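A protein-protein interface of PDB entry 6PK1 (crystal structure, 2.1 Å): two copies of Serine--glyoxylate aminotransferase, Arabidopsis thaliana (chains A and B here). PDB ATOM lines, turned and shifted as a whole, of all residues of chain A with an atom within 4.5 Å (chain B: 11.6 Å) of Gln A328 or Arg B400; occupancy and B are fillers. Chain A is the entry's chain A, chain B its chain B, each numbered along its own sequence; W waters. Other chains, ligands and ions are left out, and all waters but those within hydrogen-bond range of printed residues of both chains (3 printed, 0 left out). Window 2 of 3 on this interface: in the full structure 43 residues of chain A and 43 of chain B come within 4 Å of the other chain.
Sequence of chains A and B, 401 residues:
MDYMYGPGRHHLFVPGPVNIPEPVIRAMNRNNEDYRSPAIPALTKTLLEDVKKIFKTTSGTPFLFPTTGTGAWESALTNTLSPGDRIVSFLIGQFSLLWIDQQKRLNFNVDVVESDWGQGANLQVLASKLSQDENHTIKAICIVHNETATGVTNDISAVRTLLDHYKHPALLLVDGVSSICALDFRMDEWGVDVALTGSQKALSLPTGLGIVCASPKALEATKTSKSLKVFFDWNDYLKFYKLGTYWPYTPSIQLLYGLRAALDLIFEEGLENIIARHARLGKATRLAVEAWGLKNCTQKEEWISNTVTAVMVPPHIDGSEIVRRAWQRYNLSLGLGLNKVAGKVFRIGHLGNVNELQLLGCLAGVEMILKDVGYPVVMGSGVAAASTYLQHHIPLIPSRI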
ATOM      1  N   MET A   4     -15.824  29.003   3.623  1.00  0.00           N
ATOM      2  CA  MET A   4     -17.060  28.942   2.832  1.00  0.00           C
ATOM      3  C   MET A   4     -18.219  29.284   3.781  1.00  0.00           C
ATOM      4  O   MET A   4     -18.964  28.399   4.232  1.00  0.00           O
ATOM      5  CB  MET A   4     -17.258  27.555   2.210  1.00  0.00           C
ATOM      6  CG  MET A   4     -16.171  27.130   1.212  1.00  0.00           C
ATOM      7  SD  MET A   4     -16.424  25.398   0.673  1.00  0.00           S
ATOM      8  CE  MET A   4     -15.096  25.294  -0.566  1.00  0.00           C
ATOM      9  N   TYR A   5     -18.376  30.571   4.081  1.00  0.00           N
ATOM     10  CA  TYR A   5     -19.291  30.966   5.141  1.00  0.00           C
ATOM     11  C   TYR A   5     -20.732  30.697   4.734  1.00  0.00           C
ATOM     12  O   TYR A   5     -21.111  30.886   3.574  1.00  0.00           O
ATOM     13  CB  TYR A   5     -19.154  32.462   5.484  1.00  0.00           C
ATOM     14  CG  TYR A   5     -19.888  32.789   6.770  1.00  0.00           C
ATOM     15  CD1 TYR A   5     -21.049  33.590   6.773  1.00  0.00           C
ATOM     16  CD2 TYR A   5     -19.444  32.241   7.983  1.00  0.00           C
ATOM     17  CE1 TYR A   5     -21.726  33.864   7.964  1.00  0.00           C
ATOM     18  CE2 TYR A   5     -20.101  32.495   9.173  1.00  0.00           C
ATOM     19  CZ  TYR A   5     -21.234  33.301   9.167  1.00  0.00           C
ATOM     20  OH  TYR A   5     -21.855  33.526  10.375  1.00  0.00           O
ATOM     21  N   GLY A   6     -21.532  30.274   5.695  1.00  0.00           N
ATOM     22  CA  GLY A   6     -22.978  30.218   5.542  1.00  0.00           C
ATOM     23  C   GLY A   6     -23.638  30.800   6.771  1.00  0.00           C
ATOM     24  O   GLY A   6     -23.040  30.786   7.857  1.00  0.00           O
ATOM     25  N   ARG A 324     -24.711  16.539  -0.921  1.00  0.00           N
ATOM     26  CA  ARG A 324     -24.245  17.771  -1.527  1.00  0.00           C
ATOM     27  C   ARG A 324     -25.276  18.883  -1.334  1.00  0.00           C
ATOM     28  O   ARG A 324     -24.916  20.047  -1.097  1.00  0.00           O
ATOM     29  CB  ARG A 324     -23.979  17.547  -3.015  1.00  0.00           C
ATOM     30  CG  ARG A 324     -22.696  18.019  -3.590  1.00  0.00           C
ATOM     31  CD  ARG A 324     -22.192  17.050  -4.702  1.00  0.00           C
ATOM     32  NE  ARG A 324     -23.237  16.697  -5.667  1.00  0.00           N
ATOM     33  CZ  ARG A 324     -23.522  15.453  -6.066  1.00  0.00           C
ATOM     34  NH1 ARG A 324     -22.835  14.414  -5.606  1.00  0.00           N
ATOM     35  NH2 ARG A 324     -24.497  15.250  -6.946  1.00  0.00           N
ATOM     36  N   ARG A 325     -26.563  18.559  -1.527  1.00  0.00           N
ATOM     37  CA  ARG A 325     -27.601  19.578  -1.406  1.00  0.00           C
ATOM     38  C   ARG A 325     -27.719  20.097   0.018  1.00  0.00           C
ATOM     39  O   ARG A 325     -27.942  21.301   0.220  1.00  0.00           O
ATOM     40  CB  ARG A 325     -28.947  19.030  -1.891  1.00  0.00           C
ATOM     41  CG  ARG A 325     -29.047  19.113  -3.409  1.00  0.00           C
ATOM     42  CD  ARG A 325     -30.349  18.445  -3.922  1.00  0.00           C
ATOM     43  NE  ARG A 325     -30.362  18.342  -5.384  1.00  0.00           N
ATOM     44  CZ  ARG A 325     -30.862  19.264  -6.195  1.00  0.00           C
ATOM     45  NH1 ARG A 325     -31.417  20.376  -5.704  1.00  0.00           N
ATOM     46  NH2 ARG A 325     -30.804  19.070  -7.507  1.00  0.00           N
ATOM     47  N   ALA A 326     -27.583  19.202   1.002  1.00  0.00           N
ATOM     48  CA  ALA A 326     -27.531  19.613   2.405  1.00  0.00           C
ATOM     49  C   ALA A 326     -26.464  20.674   2.660  1.00  0.00           C
ATOM     50  O   ALA A 326     -26.720  21.660   3.367  1.00  0.00           O
ATOM     51  CB  ALA A 326     -27.282  18.412   3.288  1.00  0.00           C
ATOM     52  N   TRP A 327     -25.266  20.490   2.086  1.00  0.00           N
ATOM     53  CA  TRP A 327     -24.149  21.407   2.331  1.00  0.00           C
ATOM     54  C   TRP A 327     -24.358  22.736   1.623  1.00  0.00           C
ATOM     55  O   TRP A 327     -24.149  23.790   2.220  1.00  0.00           O
ATOM     56  CB  TRP A 327     -22.864  20.751   1.847  1.00  0.00           C
ATOM     57  CG  TRP A 327     -21.690  21.664   1.749  1.00  0.00           C
ATOM     58  CD1 TRP A 327     -21.200  22.252   0.620  1.00  0.00           C
ATOM     59  CD2 TRP A 327     -20.876  22.104   2.816  1.00  0.00           C
ATOM     60  NE1 TRP A 327     -20.102  23.009   0.913  1.00  0.00           N
ATOM     61  CE2 TRP A 327     -19.870  22.926   2.262  1.00  0.00           C
ATOM     62  CE3 TRP A 327     -20.860  21.840   4.173  1.00  0.00           C
ATOM     63  CZ2 TRP A 327     -18.870  23.527   3.034  1.00  0.00           C
ATOM     64  CZ3 TRP A 327     -19.838  22.438   4.953  1.00  0.00           C
ATOM     65  CH2 TRP A 327     -18.887  23.282   4.382  1.00  0.00           C
ATOM     66  N   GLN A 328     -24.839  22.698   0.374  1.00  0.00           N
ATOM     67  CA  GLN A 328     -24.900  23.881  -0.452  1.00  0.00           C
ATOM     68  C   GLN A 328     -26.086  24.752  -0.124  1.00  0.00           C
ATOM     69  O   GLN A 328     -26.009  25.962  -0.306  1.00  0.00           O
ATOM     70  CB  GLN A 328     -24.971  23.488  -1.945  1.00  0.00           C
ATOM     71  CG  GLN A 328     -23.684  22.936  -2.509  1.00  0.00           C
ATOM     72  CD  GLN A 328     -23.821  22.525  -3.976  1.00  0.00           C
ATOM     73  OE1 GLN A 328     -24.910  22.351  -4.480  1.00  0.00           O
ATOM     74  NE2 GLN A 328     -22.708  22.425  -4.664  1.00  0.00           N
ATOM     75  N   ARG A 329     -27.193  24.172   0.306  1.00  0.00           N
ATOM     76  CA  ARG A 329     -28.410  24.945   0.523  1.00  0.00           C
ATOM     77  C   ARG A 329     -28.825  25.053   1.991  1.00  0.00           C
ATOM     78  O   ARG A 329     -29.393  26.065   2.376  1.00  0.00           O
ATOM     79  CB  ARG A 329     -29.576  24.316  -0.256  1.00  0.00           C
ATOM     80  CG  ARG A 329     -30.808  25.212  -0.319  1.00  0.00           C
ATOM     81  CD  ARG A 329     -31.859  24.674  -1.293  1.00  0.00           C
ATOM     82  NE  ARG A 329     -32.896  25.683  -1.491  1.00  0.00           N
ATOM     83  CZ  ARG A 329     -34.138  25.445  -1.857  1.00  0.00           C
ATOM     84  NH1 ARG A 329     -34.540  24.206  -2.111  1.00  0.00           N
ATOM     85  NH2 ARG A 329     -34.973  26.446  -2.011  1.00  0.00           N
ATOM     86  N   TYR A 330     -28.610  24.015   2.805  1.00  0.00           N
ATOM     87  CA  TYR A 330     -29.168  23.985   4.138  1.00  0.00           C
ATOM     88  C   TYR A 330     -28.120  24.153   5.242  1.00  0.00           C
ATOM     89  O   TYR A 330     -28.469  24.087   6.426  1.00  0.00           O
ATOM     90  CB  TYR A 330     -29.959  22.704   4.320  1.00  0.00           C
ATOM     91  CG  TYR A 330     -31.105  22.582   3.286  1.00  0.00           C
ATOM     92  CD1 TYR A 330     -32.261  23.256   3.466  1.00  0.00           C
ATOM     93  CD2 TYR A 330     -30.944  21.828   2.138  1.00  0.00           C
ATOM     94  CE1 TYR A 330     -33.301  23.215   2.553  1.00  0.00           C
ATOM     95  CE2 TYR A 330     -31.947  21.736   1.179  1.00  0.00           C
ATOM     96  CZ  TYR A 330     -33.165  22.426   1.426  1.00  0.00           C
ATOM     97  OH  TYR A 330     -34.204  22.409   0.522  1.00  0.00           O
ATOM     98  N   ASN A 331     -26.852  24.308   4.896  1.00  0.00           N
ATOM     99  CA  ASN A 331     -25.756  24.422   5.895  1.00  0.00           C
ATOM    100  C   ASN A 331     -25.766  23.228   6.846  1.00  0.00           C
ATOM    101  O   ASN A 331     -25.732  23.357   8.064  1.00  0.00           O
ATOM    102  CB  ASN A 331     -25.833  25.738   6.661  1.00  0.00           C
ATOM    103  CG  ASN A 331     -24.466  26.213   7.221  1.00  0.00           C
ATOM    104  OD1 ASN A 331     -23.434  25.565   7.039  1.00  0.00           O
ATOM    105  ND2 ASN A 331     -24.468  27.371   7.872  1.00  0.00           N
ATOM    106  N   GLU B  22     -19.778  32.394  15.186  1.00  0.00           N
ATOM    107  CA  GLU B  22     -18.505  31.923  15.714  1.00  0.00           C
ATOM    108  C   GLU B  22     -17.342  32.796  15.321  1.00  0.00           C
ATOM    109  O   GLU B  22     -16.450  32.962  16.173  1.00  0.00           O
ATOM    110  CB  GLU B  22     -18.261  30.467  15.282  1.00  0.00           C
ATOM    111  CG  GLU B  22     -19.110  29.486  16.118  1.00  0.00           C
ATOM    112  CD  GLU B  22     -19.780  28.389  15.290  1.00  0.00           C
ATOM    113  OE1 GLU B  22     -20.626  28.708  14.425  1.00  0.00           O
ATOM    114  OE2 GLU B  22     -19.458  27.203  15.514  1.00  0.00           O
ATOM    115  N   PRO B  23     -17.227  33.312  14.083  1.00  0.00           N
ATOM    116  CA  PRO B  23     -16.094  34.209  13.767  1.00  0.00           C
ATOM    117  C   PRO B  23     -16.085  35.441  14.627  1.00  0.00           C
ATOM    118  O   PRO B  23     -15.013  35.953  14.919  1.00  0.00           O
ATOM    119  CB  PRO B  23     -16.326  34.576  12.288  1.00  0.00           C
ATOM    120  CG  PRO B  23     -17.218  33.471  11.716  1.00  0.00           C
ATOM    121  CD  PRO B  23     -18.042  32.998  12.872  1.00  0.00           C
ATOM    122  N   ARG B  26     -14.603  34.394  17.948  1.00  0.00           N
ATOM    123  CA  ARG B  26     -13.149  34.313  17.805  1.00  0.00           C
ATOM    124  C   ARG B  26     -12.516  35.706  17.855  1.00  0.00           C
ATOM    125  O   ARG B  26     -11.489  35.896  18.510  1.00  0.00           O
ATOM    126  CB  ARG B  26     -12.775  33.614  16.496  1.00  0.00           C
ATOM    127  CG  ARG B  26     -13.088  32.120  16.503  1.00  0.00           C
ATOM    128  CD  ARG B  26     -12.424  31.432  15.371  1.00  0.00           C
ATOM    129  NE  ARG B  26     -13.251  31.448  14.178  1.00  0.00           N
ATOM    130  CZ  ARG B  26     -14.287  30.653  13.988  1.00  0.00           C
ATOM    131  NH1 ARG B  26     -14.646  29.805  14.938  1.00  0.00           N
ATOM    132  NH2 ARG B  26     -14.957  30.723  12.891  1.00  0.00           N
ATOM    133  N   LEU B 265     -19.067  40.213   8.282  1.00  0.00           N
ATOM    134  CA  LEU B 265     -19.971  39.111   7.941  1.00  0.00           C
ATOM    135  C   LEU B 265     -21.218  39.632   7.270  1.00  0.00           C
ATOM    136  O   LEU B 265     -21.762  38.983   6.366  1.00  0.00           O
ATOM    137  CB  LEU B 265     -20.373  38.297   9.162  1.00  0.00           C
ATOM    138  CG  LEU B 265     -19.318  37.386   9.810  1.00  0.00           C
ATOM    139  CD1 LEU B 265     -19.963  36.624  11.019  1.00  0.00           C
ATOM    140  CD2 LEU B 265     -18.793  36.394   8.803  1.00  0.00           C
ATOM    141  N   GLU B 268     -20.410  40.446   3.752  1.00  0.00           N
ATOM    142  CA  GLU B 268     -20.173  39.235   2.972  1.00  0.00           C
ATOM    143  C   GLU B 268     -21.495  38.603   2.547  1.00  0.00           C
ATOM    144  O   GLU B 268     -21.684  38.249   1.378  1.00  0.00           O
ATOM    145  CB  GLU B 268     -19.351  38.229   3.789  1.00  0.00           C
ATOM    146  CG  GLU B 268     -18.990  36.966   3.023  1.00  0.00           C
ATOM    147  CD  GLU B 268     -17.621  36.465   3.344  1.00  0.00           C
ATOM    148  OE1 GLU B 268     -17.471  35.734   4.340  1.00  0.00           O
ATOM    149  OE2 GLU B 268     -16.686  36.830   2.609  1.00  0.00           O
ATOM    150  N   GLU B 269     -22.434  38.463   3.483  1.00  0.00           N
ATOM    151  CA  GLU B 269     -23.743  37.927   3.111  1.00  0.00           C
ATOM    152  C   GLU B 269     -24.493  38.929   2.247  1.00  0.00           C
ATOM    153  O   GLU B 269     -25.165  38.552   1.280  1.00  0.00           O
ATOM    154  CB  GLU B 269     -24.583  37.588   4.375  1.00  0.00           C
ATOM    155  CG  GLU B 269     -25.934  36.950   4.088  1.00  0.00           C
ATOM    156  CD  GLU B 269     -26.695  36.506   5.343  1.00  0.00           C
ATOM    157  OE1 GLU B 269     -26.125  36.647   6.439  1.00  0.00           O
ATOM    158  OE2 GLU B 269     -27.839  35.996   5.214  1.00  0.00           O
ATOM    159  N   ARG B 280     -37.959  35.520   5.347  1.00  0.00           N
ATOM    160  CA  ARG B 280     -38.264  34.086   5.293  1.00  0.00           C
ATOM    161  C   ARG B 280     -38.543  33.514   6.675  1.00  0.00           C
ATOM    162  O   ARG B 280     -39.465  32.706   6.860  1.00  0.00           O
ATOM    163  CB  ARG B 280     -37.115  33.283   4.647  1.00  0.00           C
ATOM    164  CG  ARG B 280     -36.929  33.519   3.223  1.00  0.00           C
ATOM    165  CD  ARG B 280     -36.025  32.417   2.638  1.00  0.00           C
ATOM    166  NE  ARG B 280     -34.728  32.351   3.286  1.00  0.00           N
ATOM    167  CZ  ARG B 280     -33.662  33.070   2.961  1.00  0.00           C
ATOM    168  NH1 ARG B 280     -33.733  33.969   2.018  1.00  0.00           N
ATOM    169  NH2 ARG B 280     -32.497  32.891   3.624  1.00  0.00           N
ATOM    170  N   ASN B 353     -28.066  36.210  13.502  1.00  0.00           N
ATOM    171  CA  ASN B 353     -27.384  35.195  12.718  1.00  0.00           C
ATOM    172  C   ASN B 353     -27.973  33.864  13.104  1.00  0.00           C
ATOM    173  O   ASN B 353     -27.542  33.213  14.039  1.00  0.00           O
ATOM    174  CB  ASN B 353     -25.888  35.253  12.939  1.00  0.00           C
ATOM    175  CG  ASN B 353     -25.139  34.601  11.838  1.00  0.00           C
ATOM    176  OD1 ASN B 353     -25.061  33.416  11.806  1.00  0.00           O
ATOM    177  ND2 ASN B 353     -24.519  35.408  10.942  1.00  0.00           N
ATOM    178  N   ASN B 355     -30.230  30.450  10.995  1.00  0.00           N
ATOM    179  CA  ASN B 355     -30.634  29.879   9.704  1.00  0.00           C
ATOM    180  C   ASN B 355     -31.906  29.077   9.878  1.00  0.00           C
ATOM    181  O   ASN B 355     -32.447  28.928  10.978  1.00  0.00           O
ATOM    182  CB  ASN B 355     -29.501  29.064   9.039  1.00  0.00           C
ATOM    183  CG  ASN B 355     -29.017  27.900   9.871  1.00  0.00           C
ATOM    184  OD1 ASN B 355     -29.793  27.183  10.505  1.00  0.00           O
ATOM    185  ND2 ASN B 355     -27.690  27.700   9.865  1.00  0.00           N
ATOM    186  N   GLU B 356     -32.394  28.576   8.747  1.00  0.00           N
ATOM    187  CA  GLU B 356     -33.715  27.969   8.689  1.00  0.00           C
ATOM    188  C   GLU B 356     -33.791  26.659   9.469  1.00  0.00           C
ATOM    189  O   GLU B 356     -34.804  26.408  10.161  1.00  0.00           O
ATOM    190  CB  GLU B 356     -34.109  27.775   7.241  1.00  0.00           C
ATOM    191  CG  GLU B 356     -34.396  29.085   6.488  1.00  0.00           C
ATOM    192  CD  GLU B 356     -33.153  29.728   5.868  1.00  0.00           C
ATOM    193  OE1 GLU B 356     -32.022  29.286   6.124  1.00  0.00           O
ATOM    194  OE2 GLU B 356     -33.316  30.687   5.125  1.00  0.00           O
ATOM    195  N   LEU B 357     -32.719  25.843   9.444  1.00  0.00           N
ATOM    196  CA  LEU B 357     -32.824  24.603  10.200  1.00  0.00           C
ATOM    197  C   LEU B 357     -32.811  24.841  11.716  1.00  0.00           C
ATOM    198  O   LEU B 357     -33.403  24.047  12.470  1.00  0.00           O
ATOM    199  CB  LEU B 357     -31.738  23.631   9.826  1.00  0.00           C
ATOM    200  CG  LEU B 357     -31.753  23.107   8.391  1.00  0.00           C
ATOM    201  CD1 LEU B 357     -30.969  21.763   8.297  1.00  0.00           C
ATOM    202  CD2 LEU B 357     -33.021  22.985   7.804  1.00  0.00           C
ATOM    203  N   GLN B 358     -32.120  25.896  12.183  1.00  0.00           N
ATOM    204  CA  GLN B 358     -32.219  26.295  13.586  1.00  0.00           C
ATOM    205  C   GLN B 358     -33.644  26.670  13.944  1.00  0.00           C
ATOM    206  O   GLN B 358     -34.191  26.223  14.963  1.00  0.00           O
ATOM    207  CB  GLN B 358     -31.312  27.483  13.900  1.00  0.00           C
ATOM    208  CG  GLN B 358     -29.830  27.118  13.965  1.00  0.00           C
ATOM    209  CD  GLN B 358     -28.965  28.399  14.065  1.00  0.00           C
ATOM    210  OE1 GLN B 358     -28.678  29.090  13.085  1.00  0.00           O
ATOM    211  NE2 GLN B 358     -28.589  28.707  15.256  1.00  0.00           N
ATOM    212  N   LEU B 390     -40.453  27.186   3.008  1.00  0.00           N
ATOM    213  CA  LEU B 390     -39.006  27.447   2.920  1.00  0.00           C
ATOM    214  C   LEU B 390     -38.342  26.675   1.803  1.00  0.00           C
ATOM    215  O   LEU B 390     -37.390  27.162   1.206  1.00  0.00           O
ATOM    216  CB  LEU B 390     -38.328  27.099   4.221  1.00  0.00           C
ATOM    217  CG  LEU B 390     -38.620  28.060   5.382  1.00  0.00           C
ATOM    218  CD1 LEU B 390     -38.073  27.465   6.643  1.00  0.00           C
ATOM    219  CD2 LEU B 390     -38.075  29.393   5.164  1.00  0.00           C
ATOM    220  N   GLN B 391     -38.815  25.470   1.503  1.00  0.00           N
ATOM    221  CA  GLN B 391     -38.240  24.692   0.419  1.00  0.00           C
ATOM    222  C   GLN B 391     -38.319  25.410  -0.906  1.00  0.00           C
ATOM    223  O   GLN B 391     -37.532  25.083  -1.811  1.00  0.00           O
ATOM    224  CB  GLN B 391     -38.959  23.326   0.335  1.00  0.00           C
ATOM    225  CG  GLN B 391     -38.399  22.358  -0.709  1.00  0.00           C
ATOM    226  CD  GLN B 391     -39.005  22.543  -2.105  1.00  0.00           C
ATOM    227  OE1 GLN B 391     -40.043  23.154  -2.235  1.00  0.00           O
ATOM    228  NE2 GLN B 391     -38.317  22.037  -3.156  1.00  0.00           N
ATOM    229  N   HIS B 393     -38.037  28.875  -1.139  1.00  0.00           N
ATOM    230  CA  HIS B 393     -37.349  30.149  -1.077  1.00  0.00           C
ATOM    231  C   HIS B 393     -35.925  30.148  -0.558  1.00  0.00           C
ATOM    232  O   HIS B 393     -35.251  31.149  -0.778  1.00  0.00           O
ATOM    233  CB  HIS B 393     -38.166  31.116  -0.221  1.00  0.00           C
ATOM    234  CG  HIS B 393     -39.462  31.486  -0.850  1.00  0.00           C
ATOM    235  ND1 HIS B 393     -40.656  30.897  -0.492  1.00  0.00           N
ATOM    236  CD2 HIS B 393     -39.741  32.334  -1.858  1.00  0.00           C
ATOM    237  CE1 HIS B 393     -41.618  31.395  -1.241  1.00  0.00           C
ATOM    238  NE2 HIS B 393     -41.090  32.278  -2.065  1.00  0.00           N
ATOM    239  N   ILE B 394     -35.465  29.115   0.148  1.00  0.00           N
ATOM    240  CA  ILE B 394     -34.085  29.198   0.641  1.00  0.00           C
ATOM    241  C   ILE B 394     -33.123  29.310  -0.543  1.00  0.00           C
ATOM    242  O   ILE B 394     -33.218  28.518  -1.494  1.00  0.00           O
ATOM    243  CB  ILE B 394     -33.730  27.987   1.502  1.00  0.00           C
ATOM    244  CG1 ILE B 394     -34.606  27.959   2.703  1.00  0.00           C
ATOM    245  CG2 ILE B 394     -32.229  28.003   1.852  1.00  0.00           C
ATOM    246  CD1 ILE B 394     -34.399  26.734   3.544  1.00  0.00           C
ATOM    247  N   PRO B 395     -32.243  30.305  -0.591  1.00  0.00           N
ATOM    248  CA  PRO B 395     -31.267  30.387  -1.681  1.00  0.00           C
ATOM    249  C   PRO B 395     -30.074  29.477  -1.430  1.00  0.00           C
ATOM    250  O   PRO B 395     -29.746  29.103  -0.302  1.00  0.00           O
ATOM    251  CB  PRO B 395     -30.817  31.852  -1.649  1.00  0.00           C
ATOM    252  CG  PRO B 395     -30.919  32.195  -0.208  1.00  0.00           C
ATOM    253  CD  PRO B 395     -32.130  31.433   0.348  1.00  0.00           C
ATOM    254  N   LEU B 396     -29.398  29.139  -2.512  1.00  0.00           N
ATOM    255  CA  LEU B 396     -28.110  28.448  -2.388  1.00  0.00           C
ATOM    256  C   LEU B 396     -27.082  29.360  -1.715  1.00  0.00           C
ATOM    257  O   LEU B 396     -27.098  30.568  -1.884  1.00  0.00           O
ATOM    258  CB  LEU B 396     -27.592  28.007  -3.773  1.00  0.00           C
ATOM    259  CG  LEU B 396     -28.543  27.039  -4.510  1.00  0.00           C
ATOM    260  CD1 LEU B 396     -28.029  26.733  -5.887  1.00  0.00           C
ATOM    261  CD2 LEU B 396     -28.736  25.764  -3.768  1.00  0.00           C
ATOM    262  N   ILE B 397     -26.174  28.766  -0.958  1.00  0.00           N
ATOM    263  CA  ILE B 397     -25.120  29.517  -0.287  1.00  0.00           C
ATOM    264  C   ILE B 397     -24.052  29.856  -1.321  1.00  0.00           C
ATOM    265  O   ILE B 397     -23.382  28.954  -1.864  1.00  0.00           O
ATOM    266  CB  ILE B 397     -24.559  28.726   0.900  1.00  0.00           C
ATOM    267  CG1 ILE B 397     -25.666  28.507   1.945  1.00  0.00           C
ATOM    268  CG2 ILE B 397     -23.359  29.450   1.544  1.00  0.00           C
ATOM    269  CD1 ILE B 397     -25.356  27.413   2.918  1.00  0.00           C
ATOM    270  N   PRO B 398     -23.882  31.145  -1.643  1.00  0.00           N
ATOM    271  CA  PRO B 398     -23.005  31.505  -2.769  1.00  0.00           C
ATOM    272  C   PRO B 398     -21.554  31.080  -2.605  1.00  0.00           C
ATOM    273  O   PRO B 398     -20.888  30.837  -3.606  1.00  0.00           O
ATOM    274  CB  PRO B 398     -23.106  33.037  -2.808  1.00  0.00           C
ATOM    275  CG  PRO B 398     -24.348  33.357  -2.099  1.00  0.00           C
ATOM    276  CD  PRO B 398     -24.604  32.316  -1.101  1.00  0.00           C
ATOM    277  N   SER B 399     -21.032  31.014  -1.374  1.00  0.00           N
ATOM    278  CA  SER B 399     -19.642  30.583  -1.162  1.00  0.00           C
ATOM    279  C   SER B 399     -19.435  29.111  -1.544  1.00  0.00           C
ATOM    280  O   SER B 399     -18.320  28.706  -1.847  1.00  0.00           O
ATOM    281  CB  SER B 399     -19.248  30.767   0.318  1.00  0.00           C
ATOM    282  OG  SER B 399     -20.149  30.031   1.180  1.00  0.00           O
ATOM    283  N   ARG B 400     -20.486  28.297  -1.529  1.00  0.00           N
ATOM    284  CA  ARG B 400     -20.395  26.872  -1.823  1.00  0.00           C
ATOM    285  C   ARG B 400     -20.810  26.570  -3.249  1.00  0.00           C
ATOM    286  O   ARG B 400     -20.926  25.391  -3.595  1.00  0.00           O
ATOM    287  CB  ARG B 400     -21.261  26.102  -0.828  1.00  0.00           C
ATOM    288  CG  ARG B 400     -20.822  26.425   0.596  1.00  0.00           C
ATOM    289  CD  ARG B 400     -21.727  25.923   1.716  1.00  0.00           C
ATOM    290  NE  ARG B 400     -21.249  26.436   2.996  1.00  0.00           N
ATOM    291  CZ  ARG B 400     -21.712  26.067   4.171  1.00  0.00           C
ATOM    292  NH1 ARG B 400     -22.668  25.120   4.257  1.00  0.00           N
ATOM    293  NH2 ARG B 400     -21.217  26.626   5.270  1.00  0.00           N
ATOM    294  N   ILE B 401     -21.009  27.622  -4.067  1.00  0.00           N
ATOM    295  CA  ILE B 401     -21.350  27.585  -5.499  1.00  0.00           C
ATOM    296  C   ILE B 401     -22.858  27.387  -5.573  1.00  0.00           C
ATOM    297  O   ILE B 401     -23.447  28.192  -6.278  1.00  0.00           O
ATOM    298  CB  ILE B 401     -20.555  26.542  -6.272  1.00  0.00           C
ATOM    299  CG1 ILE B 401     -19.054  26.789  -6.082  1.00  0.00           C
ATOM    300  CG2 ILE B 401     -20.847  26.623  -7.763  1.00  0.00           C
ATOM    301  CD1 ILE B 401     -18.660  28.261  -6.071  1.00  0.00           C
ATOM    302  OXT ILE B 401     -23.530  26.527  -4.906  1.00  0.00           O
HETATM  303  O   HOH W   1     -30.341  26.034   7.442  1.00  0.00           O
HETATM  304  O   HOH W   2     -22.008  32.740   0.933  1.00  0.00           O
HETATM  305  O   HOH W   3     -19.412  23.292  -2.205  1.00  0.00           O
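The side-chain amide nitrogen of Asn B353 sits at hydrogen-bond distance from the side-chain hydroxyl of Tyr A5 (3.3 Å). The backbone carbonyl oxygen (O) of Tyr A5 sits at hydrogen-bond distance from the side-chain hydroxyl (OG) of Ser B399 (2.7 Å). The backbone carbonyl oxygen of Trp A327 lies within hydrogen-bond range of the guanidinium group of Arg B400, 2.8 Å away. N of Ile B397 is in hydrogen-bond range of O of Gln A328 (2.9 Å). NH2 of Arg A329 sits at hydrogen-bond distance from O of Ile B394 (2.8 Å).
NH1 of Arg A329 sits at hydrogen-bond distance from OH of Tyr A330 (3.2 Å). The side-chain amide oxygen (OE1) of Gln B358 sits at hydrogen-bond distance from the backbone NH (N) of Asn B355 (2.9 Å).
Leu B265 touches Tyr A5. Ile B397 touches Tyr A5 (CG2 to O, 3.4 Å). O of Trp A327 touches CD1 of Ile B397, 3.9 Å away. O of Gln A328 touches C of Leu B396, 3.8 Å away. NE2 of Gln A328 touches O of Arg B400, at 3.6 Å. Arg A329 touches Leu B396.
Of the printed residues of chain B, Met A4 touches Ser B399 and Arg B400. Printed residues of chain B within 4 Å of Gly A6: Arg B400. No residue of chain B comes within 4 Å of Arg A325. No residue of chain B comes within 4 Å of Ala A326. Trp A327 touches two residues of chain B. Gln B358 touches none of the printed residues of chain A. His B393 touches none of the printed residues of chain A. The nearest residue of chain B that does not touch Gln A328 is Ile B401 (4.1 Å). The nearest residue of chain A that does not touch Arg B400 is Tyr A5 (4.1 Å). The nearest printed residue of chain B that does not touch Arg A329 is His B393 (4.01 Å).
Of the 11 printed residues of chain A, 8 touch a printed residue of chain B. Of the 23 printed residues of chain B, 12 touch a printed residue of chain A. Hydrophobic or aromatic side chains of chain B within 4 Å of the printed part of chain A: Pro B23, Leu B265, Leu B357, Ile B394, Leu B396 and Ile B397. Along chain B the printed residues that touch a printed residue of chain A span positions 23 to 400. Among the printed residues, no Asp or Glu carboxylate lies within 4 Å of a Lys or Arg side-chain nitrogen of the other chain.
No position is printed for both chains. Of the 22 pairs that touch across the chains among the printed residues, none has its exchanged pair printed and touching as well.
Water W3 bridges the backbone carbonyl oxygen (O) of Arg B400 and the indole nitrogen (NE1) of Trp A327. Water W2 lies within hydrogen-bond range of the backbone NH (N) of Ser B399 and the backbone carbonyl oxygen (O) of Tyr A5.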
